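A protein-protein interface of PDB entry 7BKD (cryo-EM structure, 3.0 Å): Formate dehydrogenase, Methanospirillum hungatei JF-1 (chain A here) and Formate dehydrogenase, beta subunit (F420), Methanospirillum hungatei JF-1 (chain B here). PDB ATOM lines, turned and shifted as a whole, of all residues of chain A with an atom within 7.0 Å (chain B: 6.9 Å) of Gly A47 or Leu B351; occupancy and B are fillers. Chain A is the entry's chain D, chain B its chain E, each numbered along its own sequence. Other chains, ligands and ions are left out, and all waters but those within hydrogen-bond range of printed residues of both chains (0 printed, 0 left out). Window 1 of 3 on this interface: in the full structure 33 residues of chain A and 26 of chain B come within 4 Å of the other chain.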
ATOM      1  N   THR A  23      10.397  -6.310   0.275  1.00  0.00           N
ATOM      2  CA  THR A  23       9.715  -6.487   1.545  1.00  0.00           C
ATOM      3  C   THR A  23       9.790  -7.944   1.971  1.00  0.00           C
ATOM      4  O   THR A  23       9.623  -8.850   1.152  1.00  0.00           O
ATOM      5  CB  THR A  23       8.256  -6.051   1.447  1.00  0.00           C
ATOM      6  OG1 THR A  23       8.184  -4.762   0.831  1.00  0.00           O
ATOM      7  CG2 THR A  23       7.629  -5.975   2.822  1.00  0.00           C
ATOM      8  N   LEU A  24      10.041  -8.163   3.255  1.00  0.00           N
ATOM      9  CA  LEU A  24      10.216  -9.494   3.805  1.00  0.00           C
ATOM     10  C   LEU A  24       9.575  -9.532   5.182  1.00  0.00           C
ATOM     11  O   LEU A  24       9.218  -8.498   5.745  1.00  0.00           O
ATOM     12  CB  LEU A  24      11.703  -9.867   3.828  1.00  0.00           C
ATOM     13  CG  LEU A  24      12.674  -9.018   4.652  1.00  0.00           C
ATOM     14  CD1 LEU A  24      12.714  -9.402   6.121  1.00  0.00           C
ATOM     15  CD2 LEU A  24      14.052  -9.083   4.041  1.00  0.00           C
ATOM     16  N   GLU A  37      10.735 -14.842   6.116  1.00  0.00           N
ATOM     17  CA  GLU A  37       9.684 -15.473   5.344  1.00  0.00           C
ATOM     18  C   GLU A  37       9.203 -14.543   4.242  1.00  0.00           C
ATOM     19  O   GLU A  37       9.354 -13.319   4.337  1.00  0.00           O
ATOM     20  CB  GLU A  37       8.505 -15.865   6.242  1.00  0.00           C
ATOM     21  CG  GLU A  37       8.803 -17.058   7.117  1.00  0.00           C
ATOM     22  CD  GLU A  37       9.334 -18.238   6.328  1.00  0.00           C
ATOM     23  OE1 GLU A  37       8.698 -18.622   5.326  1.00  0.00           O
ATOM     24  OE2 GLU A  37      10.390 -18.782   6.710  1.00  0.00           O
ATOM     25  N   PRO A  38       8.655 -15.100   3.168  1.00  0.00           N
ATOM     26  CA  PRO A  38       8.150 -14.260   2.083  1.00  0.00           C
ATOM     27  C   PRO A  38       6.937 -13.447   2.503  1.00  0.00           C
ATOM     28  O   PRO A  38       6.151 -13.848   3.363  1.00  0.00           O
ATOM     29  CB  PRO A  38       7.786 -15.272   0.991  1.00  0.00           C
ATOM     30  CG  PRO A  38       7.630 -16.561   1.705  1.00  0.00           C
ATOM     31  CD  PRO A  38       8.614 -16.527   2.816  1.00  0.00           C
ATOM     32  N   ASN A  39       6.797 -12.286   1.873  1.00  0.00           N
ATOM     33  CA  ASN A  39       5.649 -11.400   2.037  1.00  0.00           C
ATOM     34  C   ASN A  39       5.073 -11.184   0.642  1.00  0.00           C
ATOM     35  O   ASN A  39       5.501 -10.286  -0.085  1.00  0.00           O
ATOM     36  CB  ASN A  39       6.057 -10.092   2.693  1.00  0.00           C
ATOM     37  CG  ASN A  39       4.875  -9.232   3.060  1.00  0.00           C
ATOM     38  OD1 ASN A  39       3.904  -9.707   3.642  1.00  0.00           O
ATOM     39  ND2 ASN A  39       4.950  -7.955   2.724  1.00  0.00           N
ATOM     40  N   GLN A  40       4.100 -12.014   0.269  1.00  0.00           N
ATOM     41  CA  GLN A  40       3.572 -11.989  -1.088  1.00  0.00           C
ATOM     42  C   GLN A  40       2.737 -10.755  -1.386  1.00  0.00           C
ATOM     43  O   GLN A  40       2.476 -10.479  -2.559  1.00  0.00           O
ATOM     44  CB  GLN A  40       2.739 -13.240  -1.348  1.00  0.00           C
ATOM     45  CG  GLN A  40       3.537 -14.524  -1.346  1.00  0.00           C
ATOM     46  CD  GLN A  40       3.585 -15.161   0.017  1.00  0.00           C
ATOM     47  OE1 GLN A  40       3.464 -14.481   1.031  1.00  0.00           O
ATOM     48  NE2 GLN A  40       3.757 -16.472   0.053  1.00  0.00           N
ATOM     49  N   ARG A  41       2.307 -10.013  -0.367  1.00  0.00           N
ATOM     50  CA  ARG A  41       1.490  -8.832  -0.606  1.00  0.00           C
ATOM     51  C   ARG A  41       2.279  -7.699  -1.247  1.00  0.00           C
ATOM     52  O   ARG A  41       1.687  -6.852  -1.921  1.00  0.00           O
ATOM     53  CB  ARG A  41       0.864  -8.371   0.708  1.00  0.00           C
ATOM     54  CG  ARG A  41       0.016  -7.122   0.607  1.00  0.00           C
ATOM     55  CD  ARG A  41      -1.109  -7.285  -0.393  1.00  0.00           C
ATOM     56  NE  ARG A  41      -1.955  -6.101  -0.427  1.00  0.00           N
ATOM     57  CZ  ARG A  41      -1.652  -4.989  -1.085  1.00  0.00           C
ATOM     58  NH1 ARG A  41      -0.524  -4.908  -1.774  1.00  0.00           N
ATOM     59  NH2 ARG A  41      -2.479  -3.958  -1.056  1.00  0.00           N
ATOM     60  N   SER A  42       3.590  -7.679  -1.075  1.00  0.00           N
ATOM     61  CA  SER A  42       4.393  -6.564  -1.559  1.00  0.00           C
ATOM     62  C   SER A  42       4.367  -6.492  -3.079  1.00  0.00           C
ATOM     63  O   SER A  42       4.651  -7.490  -3.745  1.00  0.00           O
ATOM     64  CB  SER A  42       5.828  -6.707  -1.081  1.00  0.00           C
ATOM     65  OG  SER A  42       6.703  -5.971  -1.913  1.00  0.00           O
ATOM     66  N   PRO A  43       4.038  -5.340  -3.664  1.00  0.00           N
ATOM     67  CA  PRO A  43       4.129  -5.214  -5.122  1.00  0.00           C
ATOM     68  C   PRO A  43       5.551  -5.132  -5.634  1.00  0.00           C
ATOM     69  O   PRO A  43       5.764  -5.294  -6.841  1.00  0.00           O
ATOM     70  CB  PRO A  43       3.365  -3.919  -5.405  1.00  0.00           C
ATOM     71  CG  PRO A  43       3.509  -3.138  -4.165  1.00  0.00           C
ATOM     72  CD  PRO A  43       3.478  -4.131  -3.046  1.00  0.00           C
ATOM     73  N   ILE A  44       6.530  -4.878  -4.767  1.00  0.00           N
ATOM     74  CA  ILE A  44       7.900  -4.693  -5.229  1.00  0.00           C
ATOM     75  C   ILE A  44       8.505  -6.021  -5.661  1.00  0.00           C
ATOM     76  O   ILE A  44       9.108  -6.128  -6.735  1.00  0.00           O
ATOM     77  CB  ILE A  44       8.747  -4.023  -4.136  1.00  0.00           C
ATOM     78  CG1 ILE A  44       8.121  -2.697  -3.716  1.00  0.00           C
ATOM     79  CG2 ILE A  44      10.158  -3.793  -4.633  1.00  0.00           C
ATOM     80  CD1 ILE A  44       7.419  -2.756  -2.384  1.00  0.00           C
ATOM     81  N   ASN A  45       8.356  -7.053  -4.834  1.00  0.00           N
ATOM     82  CA  ASN A  45       8.990  -8.335  -5.087  1.00  0.00           C
ATOM     83  C   ASN A  45       8.043  -9.520  -5.061  1.00  0.00           C
ATOM     84  O   ASN A  45       8.476 -10.626  -5.388  1.00  0.00           O
ATOM     85  CB  ASN A  45      10.111  -8.584  -4.072  1.00  0.00           C
ATOM     86  CG  ASN A  45       9.642  -8.469  -2.650  1.00  0.00           C
ATOM     87  OD1 ASN A  45       8.842  -7.601  -2.321  1.00  0.00           O
ATOM     88  ND2 ASN A  45      10.138  -9.342  -1.792  1.00  0.00           N
ATOM     89  N   GLU A  46       6.775  -9.331  -4.702  1.00  0.00           N
ATOM     90  CA  GLU A  46       5.799 -10.419  -4.629  1.00  0.00           C
ATOM     91  C   GLU A  46       6.273 -11.556  -3.731  1.00  0.00           C
ATOM     92  O   GLU A  46       5.973 -12.723  -3.978  1.00  0.00           O
ATOM     93  CB  GLU A  46       5.438 -10.959  -6.018  1.00  0.00           C
ATOM     94  CG  GLU A  46       4.671 -10.003  -6.927  1.00  0.00           C
ATOM     95  CD  GLU A  46       5.544  -9.011  -7.674  1.00  0.00           C
ATOM     96  OE1 GLU A  46       6.781  -9.081  -7.554  1.00  0.00           O
ATOM     97  OE2 GLU A  46       4.984  -8.156  -8.394  1.00  0.00           O
ATOM     98  N   GLY A  47       7.005 -11.230  -2.673  1.00  0.00           N
ATOM     99  CA  GLY A  47       7.495 -12.236  -1.756  1.00  0.00           C
ATOM    100  C   GLY A  47       8.810 -12.876  -2.138  1.00  0.00           C
ATOM    101  O   GLY A  47       9.242 -13.817  -1.465  1.00  0.00           O
ATOM    102  N   LYS A  48       9.454 -12.400  -3.191  1.00  0.00           N
ATOM    103  CA  LYS A  48      10.666 -13.003  -3.712  1.00  0.00           C
ATOM    104  C   LYS A  48      11.876 -12.272  -3.153  1.00  0.00           C
ATOM    105  O   LYS A  48      11.836 -11.063  -2.924  1.00  0.00           O
ATOM    106  CB  LYS A  48      10.637 -12.920  -5.230  1.00  0.00           C
ATOM    107  CG  LYS A  48       9.550 -13.784  -5.797  1.00  0.00           C
ATOM    108  CD  LYS A  48       9.496 -13.749  -7.292  1.00  0.00           C
ATOM    109  CE  LYS A  48       8.361 -14.626  -7.768  1.00  0.00           C
ATOM    110  NZ  LYS A  48       8.233 -14.641  -9.236  1.00  0.00           N
ATOM    111  N   LEU A  49      12.954 -13.013  -2.911  1.00  0.00           N
ATOM    112  CA  LEU A  49      14.142 -12.429  -2.310  1.00  0.00           C
ATOM    113  C   LEU A  49      15.394 -13.040  -2.914  1.00  0.00           C
ATOM    114  O   LEU A  49      15.407 -14.203  -3.314  1.00  0.00           O
ATOM    115  CB  LEU A  49      14.173 -12.625  -0.792  1.00  0.00           C
ATOM    116  CG  LEU A  49      12.970 -12.178   0.030  1.00  0.00           C
ATOM    117  CD1 LEU A  49      12.892 -12.974   1.310  1.00  0.00           C
ATOM    118  CD2 LEU A  49      13.061 -10.703   0.324  1.00  0.00           C
ATOM    119  N   LEU A 184      16.434  -8.335  -8.166  1.00  0.00           N
ATOM    120  CA  LEU A 184      14.998  -8.274  -8.390  1.00  0.00           C
ATOM    121  C   LEU A 184      14.578  -7.050  -9.183  1.00  0.00           C
ATOM    122  O   LEU A 184      13.386  -6.885  -9.454  1.00  0.00           O
ATOM    123  CB  LEU A 184      14.243  -8.336  -7.068  1.00  0.00           C
ATOM    124  CG  LEU A 184      14.051  -9.786  -6.622  1.00  0.00           C
ATOM    125  CD1 LEU A 184      15.305 -10.354  -5.992  1.00  0.00           C
ATOM    126  CD2 LEU A 184      12.892  -9.917  -5.694  1.00  0.00           C
ATOM    127  N   THR B  77      -1.717 -17.740  -0.593  1.00  0.00           N
ATOM    128  CA  THR B  77      -1.028 -18.821  -1.291  1.00  0.00           C
ATOM    129  C   THR B  77       0.234 -19.218  -0.536  1.00  0.00           C
ATOM    130  O   THR B  77       1.351 -19.068  -1.019  1.00  0.00           O
ATOM    131  CB  THR B  77      -0.699 -18.395  -2.715  1.00  0.00           C
ATOM    132  OG1 THR B  77       0.486 -17.592  -2.704  1.00  0.00           O
ATOM    133  CG2 THR B  77      -1.828 -17.585  -3.293  1.00  0.00           C
ATOM    134  N   CYS B 296      19.274 -18.481  -5.067  1.00  0.00           N
ATOM    135  CA  CYS B 296      18.653 -17.948  -3.865  1.00  0.00           C
ATOM    136  C   CYS B 296      18.293 -19.042  -2.875  1.00  0.00           C
ATOM    137  O   CYS B 296      18.117 -18.752  -1.688  1.00  0.00           O
ATOM    138  CB  CYS B 296      17.404 -17.151  -4.227  1.00  0.00           C
ATOM    139  SG  CYS B 296      16.003 -18.165  -4.717  1.00  0.00           S
ATOM    140  N   ALA B 298      15.571 -20.424  -2.453  1.00  0.00           N
ATOM    141  CA  ALA B 298      14.216 -20.324  -1.923  1.00  0.00           C
ATOM    142  C   ALA B 298      13.351 -21.486  -2.374  1.00  0.00           C
ATOM    143  O   ALA B 298      12.387 -21.841  -1.690  1.00  0.00           O
ATOM    144  CB  ALA B 298      13.582 -19.001  -2.334  1.00  0.00           C
ATOM    145  N   CYS B 299      13.666 -22.080  -3.525  1.00  0.00           N
ATOM    146  CA  CYS B 299      12.966 -23.286  -3.951  1.00  0.00           C
ATOM    147  C   CYS B 299      13.266 -24.445  -3.019  1.00  0.00           C
ATOM    148  O   CYS B 299      12.376 -25.235  -2.693  1.00  0.00           O
ATOM    149  CB  CYS B 299      13.354 -23.640  -5.384  1.00  0.00           C
ATOM    150  SG  CYS B 299      15.117 -23.689  -5.681  1.00  0.00           S
ATOM    151  N   GLU B 301      14.370 -24.135   0.181  1.00  0.00           N
ATOM    152  CA  GLU B 301      13.940 -23.845   1.539  1.00  0.00           C
ATOM    153  C   GLU B 301      12.429 -23.878   1.694  1.00  0.00           C
ATOM    154  O   GLU B 301      11.942 -24.086   2.808  1.00  0.00           O
ATOM    155  CB  GLU B 301      14.471 -22.483   1.981  1.00  0.00           C
ATOM    156  CG  GLU B 301      15.991 -22.364   2.031  1.00  0.00           C
ATOM    157  CD  GLU B 301      16.689 -23.535   2.713  1.00  0.00           C
ATOM    158  OE1 GLU B 301      16.154 -24.074   3.705  1.00  0.00           O
ATOM    159  OE2 GLU B 301      17.789 -23.912   2.254  1.00  0.00           O
ATOM    160  N   ALA B 302      11.677 -23.678   0.615  1.00  0.00           N
ATOM    161  CA  ALA B 302      10.226 -23.635   0.707  1.00  0.00           C
ATOM    162  C   ALA B 302       9.561 -24.975   0.441  1.00  0.00           C
ATOM    163  O   ALA B 302       8.417 -25.170   0.859  1.00  0.00           O
ATOM    164  CB  ALA B 302       9.667 -22.603  -0.271  1.00  0.00           C
ATOM    165  N   GLY B 346       3.353 -25.517  -5.330  1.00  0.00           N
ATOM    166  CA  GLY B 346       3.614 -24.321  -6.093  1.00  0.00           C
ATOM    167  C   GLY B 346       4.551 -23.327  -5.453  1.00  0.00           C
ATOM    168  O   GLY B 346       4.864 -22.314  -6.082  1.00  0.00           O
ATOM    169  N   GLN B 347       5.020 -23.585  -4.233  1.00  0.00           N
ATOM    170  CA  GLN B 347       5.866 -22.617  -3.543  1.00  0.00           C
ATOM    171  C   GLN B 347       7.157 -22.367  -4.304  1.00  0.00           C
ATOM    172  O   GLN B 347       7.655 -21.238  -4.345  1.00  0.00           O
ATOM    173  CB  GLN B 347       6.175 -23.098  -2.130  1.00  0.00           C
ATOM    174  CG  GLN B 347       4.959 -23.406  -1.298  1.00  0.00           C
ATOM    175  CD  GLN B 347       4.049 -22.220  -1.150  1.00  0.00           C
ATOM    176  OE1 GLN B 347       4.505 -21.100  -0.941  1.00  0.00           O
ATOM    177  NE2 GLN B 347       2.752 -22.453  -1.259  1.00  0.00           N
ATOM    178  N   CYS B 348       7.717 -23.412  -4.908  1.00  0.00           N
ATOM    179  CA  CYS B 348       8.978 -23.272  -5.623  1.00  0.00           C
ATOM    180  C   CYS B 348       8.850 -22.301  -6.784  1.00  0.00           C
ATOM    181  O   CYS B 348       9.786 -21.555  -7.084  1.00  0.00           O
ATOM    182  CB  CYS B 348       9.443 -24.639  -6.119  1.00  0.00           C
ATOM    183  SG  CYS B 348       8.282 -25.457  -7.211  1.00  0.00           S
ATOM    184  N   GLU B 349       7.703 -22.304  -7.457  1.00  0.00           N
ATOM    185  CA  GLU B 349       7.526 -21.446  -8.617  1.00  0.00           C
ATOM    186  C   GLU B 349       7.274 -19.999  -8.230  1.00  0.00           C
ATOM    187  O   GLU B 349       7.697 -19.091  -8.951  1.00  0.00           O
ATOM    188  CB  GLU B 349       6.375 -21.960  -9.477  1.00  0.00           C
ATOM    189  CG  GLU B 349       6.407 -21.469 -10.907  1.00  0.00           C
ATOM    190  CD  GLU B 349       5.399 -22.177 -11.789  1.00  0.00           C
ATOM    191  OE1 GLU B 349       4.580 -22.954 -11.260  1.00  0.00           O
ATOM    192  OE2 GLU B 349       5.422 -21.956 -13.017  1.00  0.00           O
ATOM    193  N   GLU B 350       6.600 -19.757  -7.112  1.00  0.00           N
ATOM    194  CA  GLU B 350       6.193 -18.402  -6.771  1.00  0.00           C
ATOM    195  C   GLU B 350       7.170 -17.686  -5.857  1.00  0.00           C
ATOM    196  O   GLU B 350       6.979 -16.496  -5.592  1.00  0.00           O
ATOM    197  CB  GLU B 350       4.821 -18.409  -6.111  1.00  0.00           C
ATOM    198  CG  GLU B 350       4.793 -19.096  -4.782  1.00  0.00           C
ATOM    199  CD  GLU B 350       3.408 -19.131  -4.203  1.00  0.00           C
ATOM    200  OE1 GLU B 350       2.484 -18.632  -4.871  1.00  0.00           O
ATOM    201  OE2 GLU B 350       3.239 -19.650  -3.081  1.00  0.00           O
ATOM    202  N   LEU B 351       8.188 -18.367  -5.348  1.00  0.00           N
ATOM    203  CA  LEU B 351       9.237 -17.715  -4.584  1.00  0.00           C
ATOM    204  C   LEU B 351      10.509 -17.537  -5.392  1.00  0.00           C
ATOM    205  O   LEU B 351      11.548 -17.205  -4.821  1.00  0.00           O
ATOM    206  CB  LEU B 351       9.534 -18.501  -3.309  1.00  0.00           C
ATOM    207  CG  LEU B 351       8.393 -18.633  -2.302  1.00  0.00           C
ATOM    208  CD1 LEU B 351       8.930 -19.009  -0.942  1.00  0.00           C
ATOM    209  CD2 LEU B 351       7.597 -17.352  -2.216  1.00  0.00           C
ATOM    210  N   CYS B 352      10.451 -17.746  -6.701  1.00  0.00           N
ATOM    211  CA  CYS B 352      11.649 -17.735  -7.524  1.00  0.00           C
ATOM    212  C   CYS B 352      11.881 -16.344  -8.086  1.00  0.00           C
ATOM    213  O   CYS B 352      11.088 -15.886  -8.916  1.00  0.00           O
ATOM    214  CB  CYS B 352      11.529 -18.736  -8.656  1.00  0.00           C
ATOM    215  SG  CYS B 352      12.972 -18.844  -9.720  1.00  0.00           S
ATOM    216  N   PRO B 353      12.954 -15.659  -7.696  1.00  0.00           N
ATOM    217  CA  PRO B 353      13.199 -14.311  -8.217  1.00  0.00           C
ATOM    218  C   PRO B 353      13.327 -14.242  -9.720  1.00  0.00           C
ATOM    219  O   PRO B 353      12.999 -13.208 -10.309  1.00  0.00           O
ATOM    220  CB  PRO B 353      14.512 -13.917  -7.537  1.00  0.00           C
ATOM    221  CG  PRO B 353      14.558 -14.728  -6.327  1.00  0.00           C
ATOM    222  CD  PRO B 353      13.888 -16.011  -6.622  1.00  0.00           C
ATOM    223  N   MET B 354      13.806 -15.296 -10.365  1.00  0.00           N
ATOM    224  CA  MET B 354      14.099 -15.262 -11.788  1.00  0.00           C
ATOM    225  C   MET B 354      12.961 -15.793 -12.643  1.00  0.00           C
ATOM    226  O   MET B 354      13.119 -15.901 -13.861  1.00  0.00           O
ATOM    227  CB  MET B 354      15.383 -16.035 -12.066  1.00  0.00           C
ATOM    228  CG  MET B 354      16.635 -15.234 -11.784  1.00  0.00           C
ATOM    229  SD  MET B 354      16.486 -13.517 -12.307  1.00  0.00           S
ATOM    230  CE  MET B 354      16.897 -12.648 -10.801  1.00  0.00           C
ATOM    231  N   ASN B 358       9.394 -23.779 -11.845  1.00  0.00           N
ATOM    232  CA  ASN B 358       9.845 -24.979 -11.151  1.00  0.00           C
ATOM    233  C   ASN B 358       8.711 -25.972 -10.956  1.00  0.00           C
ATOM    234  O   ASN B 358       8.899 -27.181 -11.132  1.00  0.00           O
ATOM    235  CB  ASN B 358      10.450 -24.608  -9.803  1.00  0.00           C
ATOM    236  CG  ASN B 358      11.674 -23.750  -9.934  1.00  0.00           C
ATOM    237  OD1 ASN B 358      12.480 -23.937 -10.836  1.00  0.00           O
ATOM    238  ND2 ASN B 358      11.825 -22.803  -9.029  1.00  0.00           N
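Of the 16 printed residues of chain B, 6 touch a printed residue of chain A. Hydrophobic or aromatic side chains of chain B that line the printed part of chain A: Leu B351 and Pro B353. Among the printed residues, 10 pairs touch across the chains. Among the printed residues, no Asp or Glu carboxylate lies within 4 Å of a Lys or Arg side-chain nitrogen of the other chain.
Pro A38 touches Leu B351. Gln A40 touches Thr B77 (NE2 to O, 3.7 Å). O of Gly A47 touches CD2 of Leu B351, at 3.97 Å. O of Glu B350 touches CE of Lys A48, 3.2 Å away. Lys A48 touches Leu B351 (CG to C, 3.9 Å). Pro B353 touches Lys A48 (CA to CD, 3.9 Å). Cys B296 touches Leu A49 (CB to O, 3.7 Å). Leu A49 touches Pro B353. Pro B353 touches Leu A184.
SG of Cys B296 lies close to N of Ala B298, at 3.2 Å. The side-chain carboxylate (OE1) of Glu B350 is in hydrogen-bond range of the side-chain hydroxyl (OG1) of Thr B77, 3.1 Å away. The side-chain carboxylate (OE2) of Glu B350 sits close to the side-chain amide oxygen (OE1) of Gln B347. The backbone carbonyl oxygen (O) of Lys A48 sits at hydrogen-bond distance from the side-chain amide nitrogen (ND2) of Asn A45 (2.7 Å). O of Asn A39 is in hydrogen-bond range of N of Gly A47. SG of Cys B352 sits close to N of Met B354 (3.7 Å).
Gly A47 touches just one residue of chain B: Leu B351. Leu B351 touches just these residues of chain A: Pro A38, Gly A47 and Lys A48. Printed residues of chain A within 4 Å of Thr B77: Gln A40 (3.7 Å). Printed residues of chain B within 4 Å of Leu A184: Pro B353. Asn B358 touches none of the printed residues of chain A. The nearest residue of chain B that does not touch Gly A47 is Glu B350 (5.3 Å). The nearest residue of chain A that does not touch Leu B351 is Gln A40 (4.5 Å).
The backbone carbonyl oxygen (O) of Cys B352 lies close to the side-chain amino group (NZ) of Lys A48.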
